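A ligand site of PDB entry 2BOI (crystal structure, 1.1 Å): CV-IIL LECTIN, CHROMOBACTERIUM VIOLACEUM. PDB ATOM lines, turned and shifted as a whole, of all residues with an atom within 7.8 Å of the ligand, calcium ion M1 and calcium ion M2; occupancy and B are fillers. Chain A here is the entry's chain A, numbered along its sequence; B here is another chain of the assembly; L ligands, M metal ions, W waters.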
ATOM      1  N   VAL A  20      -4.276   7.286 -20.797  1.00  0.00           N
ATOM      2  CA  VAL A  20      -3.831   7.884 -19.553  1.00  0.00           C
ATOM      3  C   VAL A  20      -4.519   7.240 -18.345  1.00  0.00           C
ATOM      4  O   VAL A  20      -5.688   6.876 -18.389  1.00  0.00           O
ATOM      5  CB  VAL A  20      -4.021   9.407 -19.583  1.00  0.00           C
ATOM      6  CG1 VAL A  20      -3.895  10.076 -18.235  1.00  0.00           C
ATOM      7  CG2 VAL A  20      -3.032  10.023 -20.587  1.00  0.00           C
ATOM      8  N   ASN A  21      -3.740   7.109 -17.273  1.00  0.00           N
ATOM      9  CA  ASN A  21      -4.220   6.590 -15.978  1.00  0.00           C
ATOM     10  C   ASN A  21      -3.506   7.317 -14.862  1.00  0.00           C
ATOM     11  O   ASN A  21      -2.651   6.738 -14.189  1.00  0.00           O
ATOM     12  CB  ASN A  21      -3.966   5.091 -15.832  1.00  0.00           C
ATOM     13  CG  ASN A  21      -4.733   4.258 -16.824  1.00  0.00           C
ATOM     14  OD1 ASN A  21      -5.909   3.893 -16.620  1.00  0.00           O
ATOM     15  ND2 ASN A  21      -4.051   3.940 -17.948  1.00  0.00           N
ATOM     16  N   SER A  22      -3.831   8.591 -14.651  1.00  0.00           N
ATOM     17  CA  SER A  22      -3.168   9.401 -13.628  1.00  0.00           C
ATOM     18  C   SER A  22      -4.041  10.589 -13.281  1.00  0.00           C
ATOM     19  O   SER A  22      -4.821  11.073 -14.104  1.00  0.00           O
ATOM     20  CB  SER A  22      -1.828   9.901 -14.148  1.00  0.00           C
ATOM     21  OG  SER A  22      -1.168  10.617 -13.114  1.00  0.00           O
ATOM     22  N   ALA A  23      -3.870  11.065 -12.052  1.00  0.00           N
ATOM     23  CA  ALA A  23      -4.430  12.369 -11.647  1.00  0.00           C
ATOM     24  C   ALA A  23      -3.587  13.556 -12.124  1.00  0.00           C
ATOM     25  O   ALA A  23      -4.054  14.686 -12.044  1.00  0.00           O
ATOM     26  CB  ALA A  23      -4.616  12.397 -10.144  1.00  0.00           C
ATOM     27  N   ALA A  24      -2.364  13.306 -12.542  1.00  0.00           N
ATOM     28  CA  ALA A  24      -1.489  14.374 -13.022  1.00  0.00           C
ATOM     29  C   ALA A  24      -1.679  14.489 -14.534  1.00  0.00           C
ATOM     30  O   ALA A  24      -1.744  13.483 -15.255  1.00  0.00           O
ATOM     31  CB  ALA A  24      -0.082  14.049 -12.733  1.00  0.00           C
ATOM     32  N   GLN A  26      -0.778  14.621 -18.212  1.00  0.00           N
ATOM     33  CA  GLN A  26       0.259  13.997 -18.990  1.00  0.00           C
ATOM     34  C   GLN A  26       0.500  14.784 -20.257  1.00  0.00           C
ATOM     35  O   GLN A  26      -0.437  15.248 -20.885  1.00  0.00           O
ATOM     36  CB  GLN A  26      -0.176  12.576 -19.384  1.00  0.00           C
ATOM     37  CG  GLN A  26      -0.607  11.719 -18.212  1.00  0.00           C
ATOM     38  CD  GLN A  26       0.529  11.347 -17.296  1.00  0.00           C
ATOM     39  OE1 GLN A  26       1.509  10.709 -17.729  1.00  0.00           O
ATOM     40  NE2 GLN A  26       0.438  11.726 -16.007  1.00  0.00           N
ATOM     41  N   VAL A  43      -5.623  13.820 -19.002  1.00  0.00           N
ATOM     42  CA  VAL A  43      -5.633  13.428 -17.618  1.00  0.00           C
ATOM     43  C   VAL A  43      -6.796  12.488 -17.369  1.00  0.00           C
ATOM     44  O   VAL A  43      -7.757  12.507 -18.115  1.00  0.00           O
ATOM     45  CB  VAL A  43      -5.703  14.676 -16.702  1.00  0.00           C
ATOM     46  CG1 VAL A  43      -7.080  15.339 -16.778  1.00  0.00           C
ATOM     47  CG2 VAL A  43      -5.282  14.349 -15.263  1.00  0.00           C
ATOM     48  N   GLY A  44      -6.727  11.668 -16.328  1.00  0.00           N
ATOM     49  CA  GLY A  44      -7.847  10.808 -15.954  1.00  0.00           C
ATOM     50  C   GLY A  44      -7.337   9.446 -15.557  1.00  0.00           C
ATOM     51  O   GLY A  44      -6.289   9.004 -16.010  1.00  0.00           O
ATOM     52  N   THR A  45      -8.112   8.784 -14.692  1.00  0.00           N
ATOM     53  CA  THR A  45      -7.692   7.506 -14.097  1.00  0.00           C
ATOM     54  C   THR A  45      -8.374   6.311 -14.698  1.00  0.00           C
ATOM     55  O   THR A  45      -8.129   5.178 -14.229  1.00  0.00           O
ATOM     56  CB  THR A  45      -7.877   7.543 -12.566  1.00  0.00           C
ATOM     57  OG1 THR A  45      -9.218   7.877 -12.277  1.00  0.00           O
ATOM     58  CG2 THR A  45      -6.969   8.560 -11.944  1.00  0.00           C
ATOM     59  N   ASN A  69       3.905  17.005 -14.130  1.00  0.00           N
ATOM     60  CA  ASN A  69       4.430  17.777 -12.981  1.00  0.00           C
ATOM     61  C   ASN A  69       5.757  18.483 -13.323  1.00  0.00           C
ATOM     62  O   ASN A  69       6.652  18.680 -12.461  1.00  0.00           O
ATOM     63  CB  ASN A  69       4.576  16.880 -11.759  1.00  0.00           C
ATOM     64  CG  ASN A  69       3.256  16.173 -11.353  1.00  0.00           C
ATOM     65  OD1 ASN A  69       2.221  16.824 -11.163  1.00  0.00           O
ATOM     66  ND2 ASN A  69       3.299  14.870 -11.226  1.00  0.00           N
ATOM     67  N   SER A  93       4.820   4.440 -18.543  1.00  0.00           N
ATOM     68  CA  SER A  93       5.496   5.558 -17.866  1.00  0.00           C
ATOM     69  C   SER A  93       4.964   5.763 -16.475  1.00  0.00           C
ATOM     70  O   SER A  93       3.811   5.459 -16.176  1.00  0.00           O
ATOM     71  CB  SER A  93       5.365   6.826 -18.690  1.00  0.00           C
ATOM     72  OG  SER A  93       4.051   7.305 -18.752  1.00  0.00           O
ATOM     73  N   GLU A  94       5.850   6.286 -15.628  1.00  0.00           N
ATOM     74  CA  GLU A  94       5.545   6.507 -14.215  1.00  0.00           C
ATOM     75  C   GLU A  94       5.892   7.941 -13.852  1.00  0.00           C
ATOM     76  O   GLU A  94       7.028   8.395 -14.022  1.00  0.00           O
ATOM     77  CB  GLU A  94       6.356   5.527 -13.367  1.00  0.00           C
ATOM     78  CG  GLU A  94       6.123   5.679 -11.880  1.00  0.00           C
ATOM     79  CD  GLU A  94       4.679   5.611 -11.497  1.00  0.00           C
ATOM     80  OE1 GLU A  94       3.992   4.658 -11.902  1.00  0.00           O
ATOM     81  OE2 GLU A  94       4.183   6.538 -10.789  1.00  0.00           O
ATOM     82  N   ASP A  95       4.886   8.649 -13.337  1.00  0.00           N
ATOM     83  CA  ASP A  95       5.019  10.036 -12.941  1.00  0.00           C
ATOM     84  C   ASP A  95       5.192  10.228 -11.421  1.00  0.00           C
ATOM     85  O   ASP A  95       5.364  11.358 -10.967  1.00  0.00           O
ATOM     86  CB  ASP A  95       3.833  10.848 -13.469  1.00  0.00           C
ATOM     87  CG  ASP A  95       2.490  10.485 -12.852  1.00  0.00           C
ATOM     88  OD1 ASP A  95       2.432  10.163 -11.648  1.00  0.00           O
ATOM     89  OD2 ASP A  95       1.473  10.586 -13.574  1.00  0.00           O
ATOM     90  N   GLY A  96       5.108   9.146 -10.657  1.00  0.00           N
ATOM     91  CA  GLY A  96       4.970   9.248  -9.197  1.00  0.00           C
ATOM     92  C   GLY A  96       5.676   8.121  -8.474  1.00  0.00           C
ATOM     93  O   GLY A  96       6.767   7.729  -8.837  1.00  0.00           O
ATOM     94  N   THR A  97       5.010   7.617  -7.443  1.00  0.00           N
ATOM     95  CA  THR A  97       5.661   6.734  -6.455  1.00  0.00           C
ATOM     96  C   THR A  97       5.083   5.335  -6.391  1.00  0.00           C
ATOM     97  O   THR A  97       5.592   4.521  -5.635  1.00  0.00           O
ATOM     98  CB  THR A  97       5.583   7.345  -5.024  1.00  0.00           C
ATOM     99  OG1 THR A  97       4.209   7.512  -4.707  1.00  0.00           O
ATOM    100  CG2 THR A  97       6.256   8.685  -4.998  1.00  0.00           C
ATOM    101  N   ASP A  98       4.010   5.056  -7.118  1.00  0.00           N
ATOM    102  CA  ASP A  98       3.331   3.768  -6.984  1.00  0.00           C
ATOM    103  C   ASP A  98       3.818   2.711  -7.961  1.00  0.00           C
ATOM    104  O   ASP A  98       3.364   1.582  -7.897  1.00  0.00           O
ATOM    105  CB  ASP A  98       1.789   3.900  -7.036  1.00  0.00           C
ATOM    106  CG  ASP A  98       1.261   4.378  -8.370  1.00  0.00           C
ATOM    107  OD1 ASP A  98       2.086   4.815  -9.231  1.00  0.00           O
ATOM    108  OD2 ASP A  98       0.024   4.294  -8.538  1.00  0.00           O
ATOM    109  N   MET A  99       4.705   3.063  -8.891  1.00  0.00           N
ATOM    110  CA  MET A  99       5.298   2.104  -9.822  1.00  0.00           C
ATOM    111  C   MET A  99       4.245   1.305 -10.587  1.00  0.00           C
ATOM    112  O   MET A  99       4.483   0.142 -10.912  1.00  0.00           O
ATOM    113  CB  MET A  99       6.249   1.141  -9.108  1.00  0.00           C
ATOM    114  CG  MET A  99       7.334   1.768  -8.258  1.00  0.00           C
ATOM    115  SD  MET A  99       8.262   0.610  -7.256  1.00  0.00           S
ATOM    116  CE  MET A  99       7.025   0.187  -6.052  1.00  0.00           C
ATOM    117  N   ASP A 100       3.122   1.945 -10.963  1.00  0.00           N
ATOM    118  CA  ASP A 100       2.142   1.270 -11.798  1.00  0.00           C
ATOM    119  C   ASP A 100       2.427   1.363 -13.298  1.00  0.00           C
ATOM    120  O   ASP A 100       1.960   0.512 -14.073  1.00  0.00           O
ATOM    121  CB  ASP A 100       0.686   1.584 -11.447  1.00  0.00           C
ATOM    122  CG  ASP A 100       0.229   3.009 -11.720  1.00  0.00           C
ATOM    123  OD1 ASP A 100       1.047   3.858 -12.108  1.00  0.00           O
ATOM    124  OD2 ASP A 100      -0.991   3.272 -11.570  1.00  0.00           O
ATOM    125  N   TYR A 101       3.251   2.320 -13.727  1.00  0.00           N
ATOM    126  CA  TYR A 101       3.709   2.416 -15.119  1.00  0.00           C
ATOM    127  C   TYR A 101       2.589   2.499 -16.144  1.00  0.00           C
ATOM    128  O   TYR A 101       2.819   2.197 -17.329  1.00  0.00           O
ATOM    129  CB  TYR A 101       4.759   1.319 -15.443  1.00  0.00           C
ATOM    130  CG  TYR A 101       6.115   1.701 -14.847  1.00  0.00           C
ATOM    131  CD1 TYR A 101       6.969   2.506 -15.567  1.00  0.00           C
ATOM    132  CD2 TYR A 101       6.483   1.359 -13.562  1.00  0.00           C
ATOM    133  CE1 TYR A 101       8.167   3.015 -15.035  1.00  0.00           C
ATOM    134  CE2 TYR A 101       7.688   1.847 -13.009  1.00  0.00           C
ATOM    135  CZ  TYR A 101       8.499   2.665 -13.749  1.00  0.00           C
ATOM    136  OH  TYR A 101       9.665   3.140 -13.150  1.00  0.00           O
ATOM    137  N   ASN A 102       1.426   3.009 -15.740  1.00  0.00           N
ATOM    138  CA  ASN A 102       0.301   3.170 -16.644  1.00  0.00           C
ATOM    139  C   ASN A 102      -0.108   4.623 -16.819  1.00  0.00           C
ATOM    140  O   ASN A 102      -1.137   4.899 -17.400  1.00  0.00           O
ATOM    141  CB  ASN A 102      -0.893   2.332 -16.181  1.00  0.00           C
ATOM    142  CG  ASN A 102      -1.525   2.891 -14.917  1.00  0.00           C
ATOM    143  OD1 ASN A 102      -1.089   3.943 -14.432  1.00  0.00           O
ATOM    144  ND2 ASN A 102      -2.521   2.196 -14.365  1.00  0.00           N
ATOM    145  N   ASP A 103       0.719   5.549 -16.299  1.00  0.00           N
ATOM    146  CA  ASP A 103       0.256   6.926 -16.149  1.00  0.00           C
ATOM    147  C   ASP A 103      -0.020   7.561 -17.515  1.00  0.00           C
ATOM    148  O   ASP A 103      -1.042   8.205 -17.704  1.00  0.00           O
ATOM    149  CB  ASP A 103       1.242   7.692 -15.290  1.00  0.00           C
ATOM    150  CG  ASP A 103       1.342   7.142 -13.881  1.00  0.00           C
ATOM    151  OD1 ASP A 103       0.344   6.636 -13.320  1.00  0.00           O
ATOM    152  OD2 ASP A 103       2.446   7.223 -13.307  1.00  0.00           O
ATOM    153  N   SER A 104       0.921   7.340 -18.438  1.00  0.00           N
ATOM    154  CA  SER A 104       0.649   7.349 -19.877  1.00  0.00           C
ATOM    155  C   SER A 104       1.131   6.053 -20.454  1.00  0.00           C
ATOM    156  O   SER A 104       2.232   5.595 -20.093  1.00  0.00           O
ATOM    157  CB  SER A 104       1.375   8.497 -20.625  1.00  0.00           C
ATOM    158  OG  SER A 104       0.923   9.769 -20.256  1.00  0.00           O
ATOM    159  N   PRO B 111      -3.113  -3.175 -14.884  1.00  0.00           N
ATOM    160  CA  PRO B 111      -4.218  -2.514 -14.164  1.00  0.00           C
ATOM    161  C   PRO B 111      -4.393  -1.074 -14.601  1.00  0.00           C
ATOM    162  O   PRO B 111      -3.466  -0.439 -15.129  1.00  0.00           O
ATOM    163  CB  PRO B 111      -3.780  -2.595 -12.708  1.00  0.00           C
ATOM    164  CG  PRO B 111      -2.292  -2.485 -12.776  1.00  0.00           C
ATOM    165  CD  PRO B 111      -1.905  -3.276 -14.044  1.00  0.00           C
ATOM    166  N   LEU B 112      -5.559  -0.543 -14.334  1.00  0.00           N
ATOM    167  CA  LEU B 112      -5.925   0.839 -14.597  1.00  0.00           C
ATOM    168  C   LEU B 112      -5.705   1.680 -13.362  1.00  0.00           C
ATOM    169  O   LEU B 112      -5.282   1.182 -12.308  1.00  0.00           O
ATOM    170  CB  LEU B 112      -7.366   0.922 -15.067  1.00  0.00           C
ATOM    171  CG  LEU B 112      -7.705   0.024 -16.245  1.00  0.00           C
ATOM    172  CD1 LEU B 112      -9.147   0.260 -16.647  1.00  0.00           C
ATOM    173  CD2 LEU B 112      -6.764   0.266 -17.414  1.00  0.00           C
ATOM    174  N   GLY B 113      -5.980   2.971 -13.453  1.00  0.00           N
ATOM    175  CA  GLY B 113      -6.009   3.846 -12.281  1.00  0.00           C
ATOM    176  C   GLY B 113      -4.770   4.647 -12.013  1.00  0.00           C
ATOM    177  O   GLY B 113      -3.685   4.319 -12.500  1.00  0.00           O
ATOM    178  OXT GLY B 113      -4.957   5.655 -11.274  1.00  0.00           O
HETATM  179  C1  LIG L   1      -0.729   9.590  -9.946  1.00  0.00           C
HETATM  180  C2  LIG L   1      -0.216   8.301 -10.551  1.00  0.00           C
HETATM  181  C3  LIG L   1      -0.819   7.108  -9.837  1.00  0.00           C
HETATM  182  C4  LIG L   1      -2.338   7.188  -9.812  1.00  0.00           C
HETATM  183  C5  LIG L   1      -2.761   8.528  -9.235  1.00  0.00           C
HETATM  184  C6  LIG L   1      -4.271   8.688  -9.294  1.00  0.00           C
HETATM  185  O1  LIG L   1      -0.270   9.665  -8.600  1.00  0.00           O
HETATM  186  O2  LIG L   1       1.205   8.160 -10.474  1.00  0.00           O
HETATM  187  O3  LIG L   1      -0.384   5.907 -10.501  1.00  0.00           O
HETATM  188  O4  LIG L   1      -2.781   6.988 -11.171  1.00  0.00           O
HETATM  189  O5  LIG L   1      -2.158   9.599  -9.981  1.00  0.00           O
HETATM  190  C7  LIG L   1      -0.639  10.903  -7.959  1.00  0.00           C
HETATM  191 CA    CA M   1       1.929   5.914 -11.318  1.00  0.00          CA
HETATM  192 CA    CA M   2      -1.529   5.377 -12.630  1.00  0.00          CA
HETATM  193  O   HOH W   1       2.093   8.025  -7.557  1.00  0.00           O
HETATM  194  O   HOH W   2      -1.526  14.129  -8.770  1.00  0.00           O
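O of Gly 44 sits close to N of Asn 21 (3.4 Å). The backbone NH of Asp 95 lies close to the side-chain carboxylate of Asp 103. The backbone NH (N) of Asp 103 is in hydrogen-bond range of the backbone carbonyl oxygen (O) of Ser 93 (3.1 Å). The backbone NH of Gly 96 lies close to the side-chain carboxylate of Glu 94 (2.8 Å). N of Met 99 sits close to OE1 of Glu 94 (3.5 Å). NE2 of Gln 26 is in hydrogen-bond range of OD2 of Asp 95 (2.9 Å). N of Ser 22 sits at hydrogen-bond distance from O of Gly 44 (2.8 Å). The side-chain amide nitrogen (NE2) of Gln 26 sits close to the side-chain hydroxyl (OG) of Ser 22, 3.5 Å away.
Calcium ion M2 is bound by OD1 of Asn 102 (2.3 Å). Calcium ion M2 is bound by the backbone carbonyl oxygen (O) of Asn 21 (2.4 Å). OD1 of Asp 103 binds calcium ion M2 (2.4 Å). O of Gly 113 of chain B binds calcium ion M2 (2.4 Å). Calcium ion M2 is bound by the side-chain carboxylate (OD2) of Asp 100 (2.4 Å). Calcium ion M2 is bound by an oxygen (O3) of the ligand, at 2.5 Å. O4 of the ligand is bound to calcium ion M2 (2.5 Å). Calcium ion M2 has seven donor atoms within binding distance. Slightly farther from calcium ion M2 lies OD1 of Asp 100 (3.0 Å).
Residues that only touch the ligand: Thr 45 (3.8 Å). Hydrophobic or aromatic side chains that line the ligand: Ala 23. Ten residues have an atom within 4 Å of the ligand: Asn 21, Ser 22, Ala 23, Thr 45, Glu 94, Asp 95, Asp 98, Asp 100, Asp 103 and Gly 113 of chain B. The nearest printed residue that does not touch the ligand is Gly 96 (4.03 Å).
Of the 25 residues printed, 4 come within 4 Å of calcium ion M1. The nearest printed residue that does not touch calcium ion M1 is Asp 95 (4.3 Å).
Water W1 lies within hydrogen-bond range of the backbone NH (N) of Thr 97 (2.9 Å) and an oxygen (O1) of the ligand (3.1 Å).
Calcium ion M1 is bound by the side-chain carboxylate (OD1) of Asp 98, 2.4 Å away. Calcium ion M1 is bound by OD1 of Asp 100, 2.4 Å away. OE2 of Glu 94 binds calcium ion M1 (2.4 Å). Calcium ion M1 is bound by OD2 of Asp 103, at 2.4 Å. Calcium ion M1 is bound by O3 of the ligand, at 2.5 Å. OE1 of Glu 94 binds calcium ion M1, at 2.5 Å. An oxygen (O2) of the ligand binds calcium ion M1 (2.5 Å). Calcium ion M1 is bound by OD1 of Asp 103 (2.7 Å). Calcium ion M1 has eight donor atoms within binding distance.
OD1 of Asp 95 lies close to O2 of the ligand (2.6 Å). The backbone NH of Ala 23 sits at hydrogen-bond distance from an oxygen (O5) of the ligand (3.1 Å). OG of Ser 22 sits close to O5 of the ligand, at 3.4 Å.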
